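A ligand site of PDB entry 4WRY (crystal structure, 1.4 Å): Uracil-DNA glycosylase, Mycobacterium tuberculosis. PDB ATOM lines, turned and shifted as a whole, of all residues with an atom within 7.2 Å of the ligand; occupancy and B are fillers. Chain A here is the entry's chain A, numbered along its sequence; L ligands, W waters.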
ATOM      1  N   VAL A  76     -30.269 -20.442   1.051  1.00  0.00           N
ATOM      2  CA  VAL A  76     -30.080 -21.616   0.211  1.00  0.00           C
ATOM      3  C   VAL A  76     -28.647 -21.585  -0.310  1.00  0.00           C
ATOM      4  O   VAL A  76     -28.194 -20.625  -0.939  1.00  0.00           O
ATOM      5  CB  VAL A  76     -31.051 -21.684  -0.976  1.00  0.00           C
ATOM      6  CG1 VAL A  76     -30.943 -23.012  -1.718  1.00  0.00           C
ATOM      7  CG2 VAL A  76     -32.481 -21.516  -0.486  1.00  0.00           C
ATOM      8  N   GLY A  77     -27.953 -22.704  -0.094  1.00  0.00           N
ATOM      9  CA  GLY A  77     -26.654 -22.958  -0.702  1.00  0.00           C
ATOM     10  C   GLY A  77     -26.732 -24.129  -1.689  1.00  0.00           C
ATOM     11  O   GLY A  77     -27.791 -24.525  -2.151  1.00  0.00           O
ATOM     12  N   GLN A  78     -25.548 -24.627  -2.007  1.00  0.00           N
ATOM     13  CA  GLN A  78     -25.373 -25.580  -3.045  1.00  0.00           C
ATOM     14  C   GLN A  78     -25.595 -27.054  -2.539  1.00  0.00           C
ATOM     15  O   GLN A  78     -26.469 -27.752  -3.018  1.00  0.00           O
ATOM     16  CB  GLN A  78     -23.959 -25.447  -3.640  1.00  0.00           C
ATOM     17  CG  GLN A  78     -23.656 -26.510  -4.665  1.00  0.00           C
ATOM     18  CD  GLN A  78     -22.247 -26.366  -5.207  1.00  0.00           C
ATOM     19  OE1 GLN A  78     -21.301 -27.113  -4.834  1.00  0.00           O
ATOM     20  NE2 GLN A  78     -22.092 -25.470  -6.090  1.00  0.00           N
ATOM     21  N   ASP A  79     -24.726 -27.463  -1.661  1.00  0.00           N
ATOM     22  CA  ASP A  79     -24.662 -28.803  -1.129  1.00  0.00           C
ATOM     23  C   ASP A  79     -23.806 -28.765   0.126  1.00  0.00           C
ATOM     24  O   ASP A  79     -23.188 -27.740   0.490  1.00  0.00           O
ATOM     25  CB  ASP A  79     -24.142 -29.812  -2.171  1.00  0.00           C
ATOM     26  CG  ASP A  79     -22.700 -29.686  -2.521  1.00  0.00           C
ATOM     27  OD1 ASP A  79     -22.062 -28.637  -2.438  1.00  0.00           O
ATOM     28  OD2 ASP A  79     -22.140 -30.744  -2.937  1.00  0.00           O
ATOM     29  N   PRO A  80     -23.809 -29.861   0.902  1.00  0.00           N
ATOM     30  CA  PRO A  80     -23.136 -29.795   2.204  1.00  0.00           C
ATOM     31  C   PRO A  80     -21.621 -29.614   2.141  1.00  0.00           C
ATOM     32  O   PRO A  80     -21.004 -29.974   1.120  1.00  0.00           O
ATOM     33  CB  PRO A  80     -23.470 -31.138   2.868  1.00  0.00           C
ATOM     34  CG  PRO A  80     -24.792 -31.568   2.181  1.00  0.00           C
ATOM     35  CD  PRO A  80     -24.588 -31.107   0.752  1.00  0.00           C
ATOM     36  N   TYR A  81     -21.081 -29.108   3.214  1.00  0.00           N
ATOM     37  CA  TYR A  81     -19.626 -29.096   3.351  1.00  0.00           C
ATOM     38  C   TYR A  81     -19.051 -30.489   3.023  1.00  0.00           C
ATOM     39  O   TYR A  81     -19.583 -31.522   3.476  1.00  0.00           O
ATOM     40  CB  TYR A  81     -19.186 -28.783   4.776  1.00  0.00           C
ATOM     41  CG  TYR A  81     -19.373 -27.351   5.198  1.00  0.00           C
ATOM     42  CD1 TYR A  81     -18.752 -26.324   4.470  1.00  0.00           C
ATOM     43  CD2 TYR A  81     -20.217 -27.028   6.267  1.00  0.00           C
ATOM     44  CE1 TYR A  81     -18.928 -24.985   4.841  1.00  0.00           C
ATOM     45  CE2 TYR A  81     -20.409 -25.690   6.622  1.00  0.00           C
ATOM     46  CZ  TYR A  81     -19.753 -24.674   5.917  1.00  0.00           C
ATOM     47  OH  TYR A  81     -19.930 -23.354   6.302  1.00  0.00           O
ATOM     48  N   PRO A  82     -17.971 -30.535   2.245  1.00  0.00           N
ATOM     49  CA  PRO A  82     -17.400 -31.833   1.820  1.00  0.00           C
ATOM     50  C   PRO A  82     -16.419 -32.419   2.831  1.00  0.00           C
ATOM     51  O   PRO A  82     -16.040 -33.578   2.701  1.00  0.00           O
ATOM     52  CB  PRO A  82     -16.675 -31.458   0.532  1.00  0.00           C
ATOM     53  CG  PRO A  82     -16.191 -30.040   0.790  1.00  0.00           C
ATOM     54  CD  PRO A  82     -17.334 -29.403   1.538  1.00  0.00           C
ATOM     55  N   ALA A  87     -20.309 -30.811   7.832  1.00  0.00           N
ATOM     56  CA  ALA A  87     -21.737 -30.797   7.484  1.00  0.00           C
ATOM     57  C   ALA A  87     -22.598 -31.394   8.582  1.00  0.00           C
ATOM     58  O   ALA A  87     -22.332 -32.501   9.095  1.00  0.00           O
ATOM     59  CB  ALA A  87     -22.017 -31.553   6.187  1.00  0.00           C
ATOM     60  N   VAL A  88     -23.670 -30.685   8.963  1.00  0.00           N
ATOM     61  CA  VAL A  88     -24.547 -31.154  10.014  1.00  0.00           C
ATOM     62  C   VAL A  88     -26.017 -31.063   9.604  1.00  0.00           C
ATOM     63  O   VAL A  88     -26.906 -31.114  10.469  1.00  0.00           O
ATOM     64  CB  VAL A  88     -24.321 -30.385  11.335  1.00  0.00           C
ATOM     65  CG1 VAL A  88     -22.897 -30.691  11.823  1.00  0.00           C
ATOM     66  CG2 VAL A  88     -24.567 -28.901  11.179  1.00  0.00           C
ATOM     67  N   GLY A  89     -26.294 -30.859   8.318  1.00  0.00           N
ATOM     68  CA  GLY A  89     -27.670 -30.855   7.852  1.00  0.00           C
ATOM     69  C   GLY A  89     -28.380 -29.524   7.860  1.00  0.00           C
ATOM     70  O   GLY A  89     -29.546 -29.414   7.477  1.00  0.00           O
ATOM     71  N   LEU A  90     -27.695 -28.493   8.362  1.00  0.00           N
ATOM     72  CA  LEU A  90     -28.175 -27.111   8.234  1.00  0.00           C
ATOM     73  C   LEU A  90     -27.184 -26.399   7.356  1.00  0.00           C
ATOM     74  O   LEU A  90     -25.970 -26.405   7.678  1.00  0.00           O
ATOM     75  CB  LEU A  90     -28.267 -26.432   9.626  1.00  0.00           C
ATOM     76  CG  LEU A  90     -29.231 -27.035  10.607  1.00  0.00           C
ATOM     77  CD1 LEU A  90     -29.142 -26.316  11.931  1.00  0.00           C
ATOM     78  CD2 LEU A  90     -30.620 -26.945  10.100  1.00  0.00           C
ATOM     79  N   SER A  91     -27.620 -25.779   6.271  1.00  0.00           N
ATOM     80  CA  SER A  91     -26.668 -25.211   5.310  1.00  0.00           C
ATOM     81  C   SER A  91     -25.775 -24.201   6.030  1.00  0.00           C
ATOM     82  O   SER A  91     -26.209 -23.347   6.830  1.00  0.00           O
ATOM     83  CB  SER A  91     -27.346 -24.591   4.136  1.00  0.00           C
ATOM     84  OG  SER A  91     -28.211 -23.534   4.512  1.00  0.00           O
ATOM     85  N   PHE A  92     -24.490 -24.338   5.691  1.00  0.00           N
ATOM     86  CA  PHE A  92     -23.424 -23.492   6.188  1.00  0.00           C
ATOM     87  C   PHE A  92     -22.981 -23.641   7.629  1.00  0.00           C
ATOM     88  O   PHE A  92     -21.915 -23.109   8.048  1.00  0.00           O
ATOM     89  CB  PHE A  92     -23.630 -22.041   5.795  1.00  0.00           C
ATOM     90  CG  PHE A  92     -23.783 -21.856   4.351  1.00  0.00           C
ATOM     91  CD1 PHE A  92     -22.661 -21.820   3.549  1.00  0.00           C
ATOM     92  CD2 PHE A  92     -25.029 -21.717   3.787  1.00  0.00           C
ATOM     93  CE1 PHE A  92     -22.778 -21.615   2.186  1.00  0.00           C
ATOM     94  CE2 PHE A  92     -25.180 -21.569   2.421  1.00  0.00           C
ATOM     95  CZ  PHE A  92     -24.041 -21.522   1.634  1.00  0.00           C
ATOM     96  N   SER A  93     -23.775 -24.351   8.411  1.00  0.00           N
ATOM     97  CA  SER A  93     -23.539 -24.487   9.855  1.00  0.00           C
ATOM     98  C   SER A  93     -22.470 -25.517  10.153  1.00  0.00           C
ATOM     99  O   SER A  93     -22.284 -26.472   9.374  1.00  0.00           O
ATOM    100  CB  SER A  93     -24.823 -24.912  10.541  1.00  0.00           C
ATOM    101  OG  SER A  93     -24.771 -24.769  11.943  1.00  0.00           O
ATOM    102  N   PRO A 102     -14.993 -23.449   8.397  1.00  0.00           N
ATOM    103  CA  PRO A 102     -14.857 -23.426   6.939  1.00  0.00           C
ATOM    104  C   PRO A 102     -14.782 -21.983   6.416  1.00  0.00           C
ATOM    105  O   PRO A 102     -15.406 -21.077   6.957  1.00  0.00           O
ATOM    106  CB  PRO A 102     -16.112 -24.161   6.436  1.00  0.00           C
ATOM    107  CG  PRO A 102     -16.543 -24.929   7.586  1.00  0.00           C
ATOM    108  CD  PRO A 102     -16.168 -24.190   8.818  1.00  0.00           C
ATOM    109  N   SER A 104     -16.099 -20.545   3.849  1.00  0.00           N
ATOM    110  CA  SER A 104     -17.397 -19.968   3.474  1.00  0.00           C
ATOM    111  C   SER A 104     -18.035 -19.348   4.702  1.00  0.00           C
ATOM    112  O   SER A 104     -18.628 -18.301   4.615  1.00  0.00           O
ATOM    113  CB  SER A 104     -18.347 -21.041   2.916  1.00  0.00           C
ATOM    114  OG  SER A 104     -17.997 -21.435   1.608  1.00  0.00           O
ATOM    115  N   LEU A 105     -17.973 -20.044   5.830  1.00  0.00           N
ATOM    116  CA  LEU A 105     -18.590 -19.538   7.069  1.00  0.00           C
ATOM    117  C   LEU A 105     -17.846 -18.367   7.649  1.00  0.00           C
ATOM    118  O   LEU A 105     -18.446 -17.424   8.083  1.00  0.00           O
ATOM    119  CB  LEU A 105     -18.714 -20.683   8.075  1.00  0.00           C
ATOM    120  CG  LEU A 105     -19.493 -20.392   9.351  1.00  0.00           C
ATOM    121  CD1 LEU A 105     -20.892 -19.957   9.068  1.00  0.00           C
ATOM    122  CD2 LEU A 105     -19.481 -21.621  10.300  1.00  0.00           C
ATOM    123  N   ILE A 108     -19.176 -15.630   5.592  1.00  0.00           N
ATOM    124  CA  ILE A 108     -20.501 -15.277   6.056  1.00  0.00           C
ATOM    125  C   ILE A 108     -20.416 -14.412   7.328  1.00  0.00           C
ATOM    126  O   ILE A 108     -21.127 -13.430   7.452  1.00  0.00           O
ATOM    127  CB  ILE A 108     -21.362 -16.509   6.284  1.00  0.00           C
ATOM    128  CG1 ILE A 108     -21.746 -17.181   4.962  1.00  0.00           C
ATOM    129  CG2 ILE A 108     -22.602 -16.188   7.076  1.00  0.00           C
ATOM    130  CD1 ILE A 108     -22.144 -18.665   5.067  1.00  0.00           C
ATOM    131  N   LEU A 136     -32.427 -23.319   6.614  1.00  0.00           N
ATOM    132  CA  LEU A 136     -31.045 -23.380   6.216  1.00  0.00           C
ATOM    133  C   LEU A 136     -30.876 -24.552   5.213  1.00  0.00           C
ATOM    134  O   LEU A 136     -30.500 -25.682   5.594  1.00  0.00           O
ATOM    135  CB  LEU A 136     -30.129 -23.504   7.427  1.00  0.00           C
ATOM    136  CG  LEU A 136     -30.216 -22.351   8.399  1.00  0.00           C
ATOM    137  CD1 LEU A 136     -29.385 -22.655   9.629  1.00  0.00           C
ATOM    138  CD2 LEU A 136     -29.798 -21.098   7.767  1.00  0.00           C
ATOM    139  N   LEU A 137     -31.251 -24.271   3.974  1.00  0.00           N
ATOM    140  CA  LEU A 137     -31.386 -25.272   2.915  1.00  0.00           C
ATOM    141  C   LEU A 137     -30.187 -25.308   2.018  1.00  0.00           C
ATOM    142  O   LEU A 137     -29.499 -24.315   1.801  1.00  0.00           O
ATOM    143  CB  LEU A 137     -32.616 -24.906   2.101  1.00  0.00           C
ATOM    144  CG  LEU A 137     -33.083 -25.930   1.076  1.00  0.00           C
ATOM    145  CD1 LEU A 137     -33.544 -27.207   1.765  1.00  0.00           C
ATOM    146  CD2 LEU A 137     -34.174 -25.341   0.253  1.00  0.00           C
ATOM    147  N   ASN A 138     -29.892 -26.493   1.527  1.00  0.00           N
ATOM    148  CA  ASN A 138     -29.058 -26.665   0.375  1.00  0.00           C
ATOM    149  C   ASN A 138     -29.898 -27.220  -0.764  1.00  0.00           C
ATOM    150  O   ASN A 138     -30.844 -27.969  -0.564  1.00  0.00           O
ATOM    151  CB  ASN A 138     -27.867 -27.592   0.613  1.00  0.00           C
ATOM    152  CG  ASN A 138     -26.753 -26.920   1.364  1.00  0.00           C
ATOM    153  OD1 ASN A 138     -26.349 -25.756   1.001  1.00  0.00           O
ATOM    154  ND2 ASN A 138     -26.271 -27.574   2.367  1.00  0.00           N
ATOM    155  N   ARG A 139     -29.523 -26.872  -2.003  1.00  0.00           N
ATOM    156  CA  ARG A 139     -30.272 -27.363  -3.167  1.00  0.00           C
ATOM    157  C   ARG A 139     -30.174 -28.914  -3.211  1.00  0.00           C
ATOM    158  O   ARG A 139     -31.113 -29.608  -3.620  1.00  0.00           O
ATOM    159  CB  ARG A 139     -29.639 -26.761  -4.422  1.00  0.00           C
ATOM    160  CG  ARG A 139     -30.420 -26.870  -5.614  1.00  0.00           C
ATOM    161  CD  ARG A 139     -31.669 -25.994  -5.576  1.00  0.00           C
ATOM    162  NE  ARG A 139     -32.287 -26.115  -6.906  1.00  0.00           N
ATOM    163  CZ  ARG A 139     -33.295 -26.927  -7.235  1.00  0.00           C
ATOM    164  NH1 ARG A 139     -33.930 -27.781  -6.372  1.00  0.00           N
ATOM    165  NH2 ARG A 139     -33.682 -26.876  -8.499  1.00  0.00           N
ATOM    166  N   VAL A 140     -28.998 -29.426  -2.875  1.00  0.00           N
ATOM    167  CA  VAL A 140     -28.718 -30.882  -2.817  1.00  0.00           C
ATOM    168  C   VAL A 140     -28.327 -31.185  -1.411  1.00  0.00           C
ATOM    169  O   VAL A 140     -27.519 -30.478  -0.779  1.00  0.00           O
ATOM    170  CB  VAL A 140     -27.597 -31.207  -3.827  1.00  0.00           C
ATOM    171  CG1 VAL A 140     -27.057 -32.601  -3.661  1.00  0.00           C
ATOM    172  CG2 VAL A 140     -28.167 -31.028  -5.216  1.00  0.00           C
ATOM    173  N   TRP A 179     -27.553 -18.093  -2.290  1.00  0.00           N
ATOM    174  CA  TRP A 179     -26.113 -17.964  -2.356  1.00  0.00           C
ATOM    175  C   TRP A 179     -25.539 -18.927  -3.388  1.00  0.00           C
ATOM    176  O   TRP A 179     -25.447 -20.158  -3.175  1.00  0.00           O
ATOM    177  CB  TRP A 179     -25.470 -18.170  -0.993  1.00  0.00           C
ATOM    178  CG  TRP A 179     -25.678 -17.022  -0.039  1.00  0.00           C
ATOM    179  CD1 TRP A 179     -25.961 -15.711  -0.368  1.00  0.00           C
ATOM    180  CD2 TRP A 179     -25.592 -17.054   1.391  1.00  0.00           C
ATOM    181  NE1 TRP A 179     -26.068 -14.946   0.763  1.00  0.00           N
ATOM    182  CE2 TRP A 179     -25.849 -15.723   1.869  1.00  0.00           C
ATOM    183  CE3 TRP A 179     -25.285 -18.064   2.329  1.00  0.00           C
ATOM    184  CZ2 TRP A 179     -25.859 -15.415   3.221  1.00  0.00           C
ATOM    185  CZ3 TRP A 179     -25.336 -17.783   3.665  1.00  0.00           C
ATOM    186  CH2 TRP A 179     -25.583 -16.470   4.112  1.00  0.00           C
ATOM    187  N   HIS A 202     -21.824 -16.896  -4.221  1.00  0.00           N
ATOM    188  CA  HIS A 202     -21.592 -17.742  -3.088  1.00  0.00           C
ATOM    189  C   HIS A 202     -20.496 -17.185  -2.146  1.00  0.00           C
ATOM    190  O   HIS A 202     -19.557 -16.574  -2.638  1.00  0.00           O
ATOM    191  CB  HIS A 202     -21.241 -19.125  -3.648  1.00  0.00           C
ATOM    192  CG  HIS A 202     -21.260 -20.257  -2.653  1.00  0.00           C
ATOM    193  ND1 HIS A 202     -20.215 -20.502  -1.796  1.00  0.00           N
ATOM    194  CD2 HIS A 202     -22.211 -21.175  -2.373  1.00  0.00           C
ATOM    195  CE1 HIS A 202     -20.515 -21.552  -1.028  1.00  0.00           C
ATOM    196  NE2 HIS A 202     -21.731 -21.974  -1.379  1.00  0.00           N
ATOM    197  N   PRO A 203     -20.573 -17.452  -0.835  1.00  0.00           N
ATOM    198  CA  PRO A 203     -19.570 -16.906   0.081  1.00  0.00           C
ATOM    199  C   PRO A 203     -18.234 -17.622   0.089  1.00  0.00           C
ATOM    200  O   PRO A 203     -17.321 -17.152   0.749  1.00  0.00           O
ATOM    201  CB  PRO A 203     -20.238 -16.988   1.435  1.00  0.00           C
ATOM    202  CG  PRO A 203     -21.217 -18.147   1.255  1.00  0.00           C
ATOM    203  CD  PRO A 203     -21.744 -17.981  -0.113  1.00  0.00           C
ATOM    204  N   SER A 204     -18.072 -18.759  -0.634  1.00  0.00           N
ATOM    205  CA  SER A 204     -16.764 -19.353  -0.711  1.00  0.00           C
ATOM    206  C   SER A 204     -15.710 -18.363  -1.229  1.00  0.00           C
ATOM    207  O   SER A 204     -16.007 -17.524  -2.029  1.00  0.00           O
ATOM    208  CB  SER A 204     -16.819 -20.625  -1.563  1.00  0.00           C
ATOM    209  OG  SER A 204     -17.011 -20.256  -2.940  1.00  0.00           O
HETATM  210  N1  LIG L   1     -21.880 -25.591   3.199  1.00  0.00           N
HETATM  211  C1  LIG L   1     -23.187 -25.680   2.791  1.00  0.00           C
HETATM  212  N2  LIG L   1     -23.657 -25.107   1.650  1.00  0.00           N
HETATM  213  C2  LIG L   1     -22.858 -24.616   0.648  1.00  0.00           C
HETATM  214  C3  LIG L   1     -21.449 -24.586   1.047  1.00  0.00           C
HETATM  215  C4  LIG L   1     -21.061 -25.132   2.260  1.00  0.00           C
HETATM  216  O1  LIG L   1     -24.043 -26.142   3.583  1.00  0.00           O
HETATM  217  O2  LIG L   1     -23.245 -24.160  -0.446  1.00  0.00           O
HETATM  218  F1  LIG L   1     -20.503 -24.065   0.315  1.00  0.00           F
HETATM  219  O   HOH W   1     -23.308 -28.090   5.079  1.00  0.00           O
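An oxygen (O1) of the ligand lies within hydrogen-bond range of the backbone NH (N) of Phe 92, 2.8 Å away. The backbone carbonyl oxygen of Asp 79 lies within hydrogen-bond range of a nitrogen (N2) of the ligand, at 2.9 Å. The backbone NH (N) of Gln 78 lies within hydrogen-bond range of an oxygen (O2) of the ligand (2.8 Å). A nitrogen (N2) of the ligand lies within hydrogen-bond range of the side-chain amide oxygen (OD1) of Asn 138. NE2 of His 202 is in hydrogen-bond range of O2 of the ligand (2.8 Å).
The backbone NH (N) of Gly 77 is in hydrogen-bond range of the backbone carbonyl oxygen (O) of Leu 137. N of Ser 204 sits close to OG of Ser 104. OD1 of Asn 138 is in hydrogen-bond range of N of Gln 78 (3.3 Å). The backbone carbonyl oxygen (O) of Phe 92 sits at hydrogen-bond distance from the side-chain hydroxyl (OH) of Tyr 81, at 2.7 Å. OE1 of Gln 78 sits close to OD1 of Asp 79. The backbone NH (N) of Arg 139 lies within hydrogen-bond range of the backbone carbonyl oxygen (O) of Gly 77 (2.9 Å). O of Leu 136 lies within hydrogen-bond range of N of Ser 91 (3.0 Å). The backbone carbonyl oxygen of Gln 78 is in hydrogen-bond range of the backbone NH of Val 140 (3.0 Å).
Residues that only touch the ligand: Ser 91 (3.3 Å), Tyr 81 (3.4 Å), Gly 77 (3.6 Å) and Ser 104 (3.9 Å). Hydrophobic or aromatic side chains within 4 Å of the ligand: Tyr 81, Phe 92 and His 202. Within 4 Å of the ligand: Gly 77, Gln 78, Asp 79, Tyr 81, Ser 91, Phe 92, Ser 104, Asn 138 and His 202. The nearest printed residue that does not touch the ligand is Pro 80 (4.01 Å).
Water W1 bridges O1 of the ligand (2.6 Å) and N of Tyr 81 (3.1 Å).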
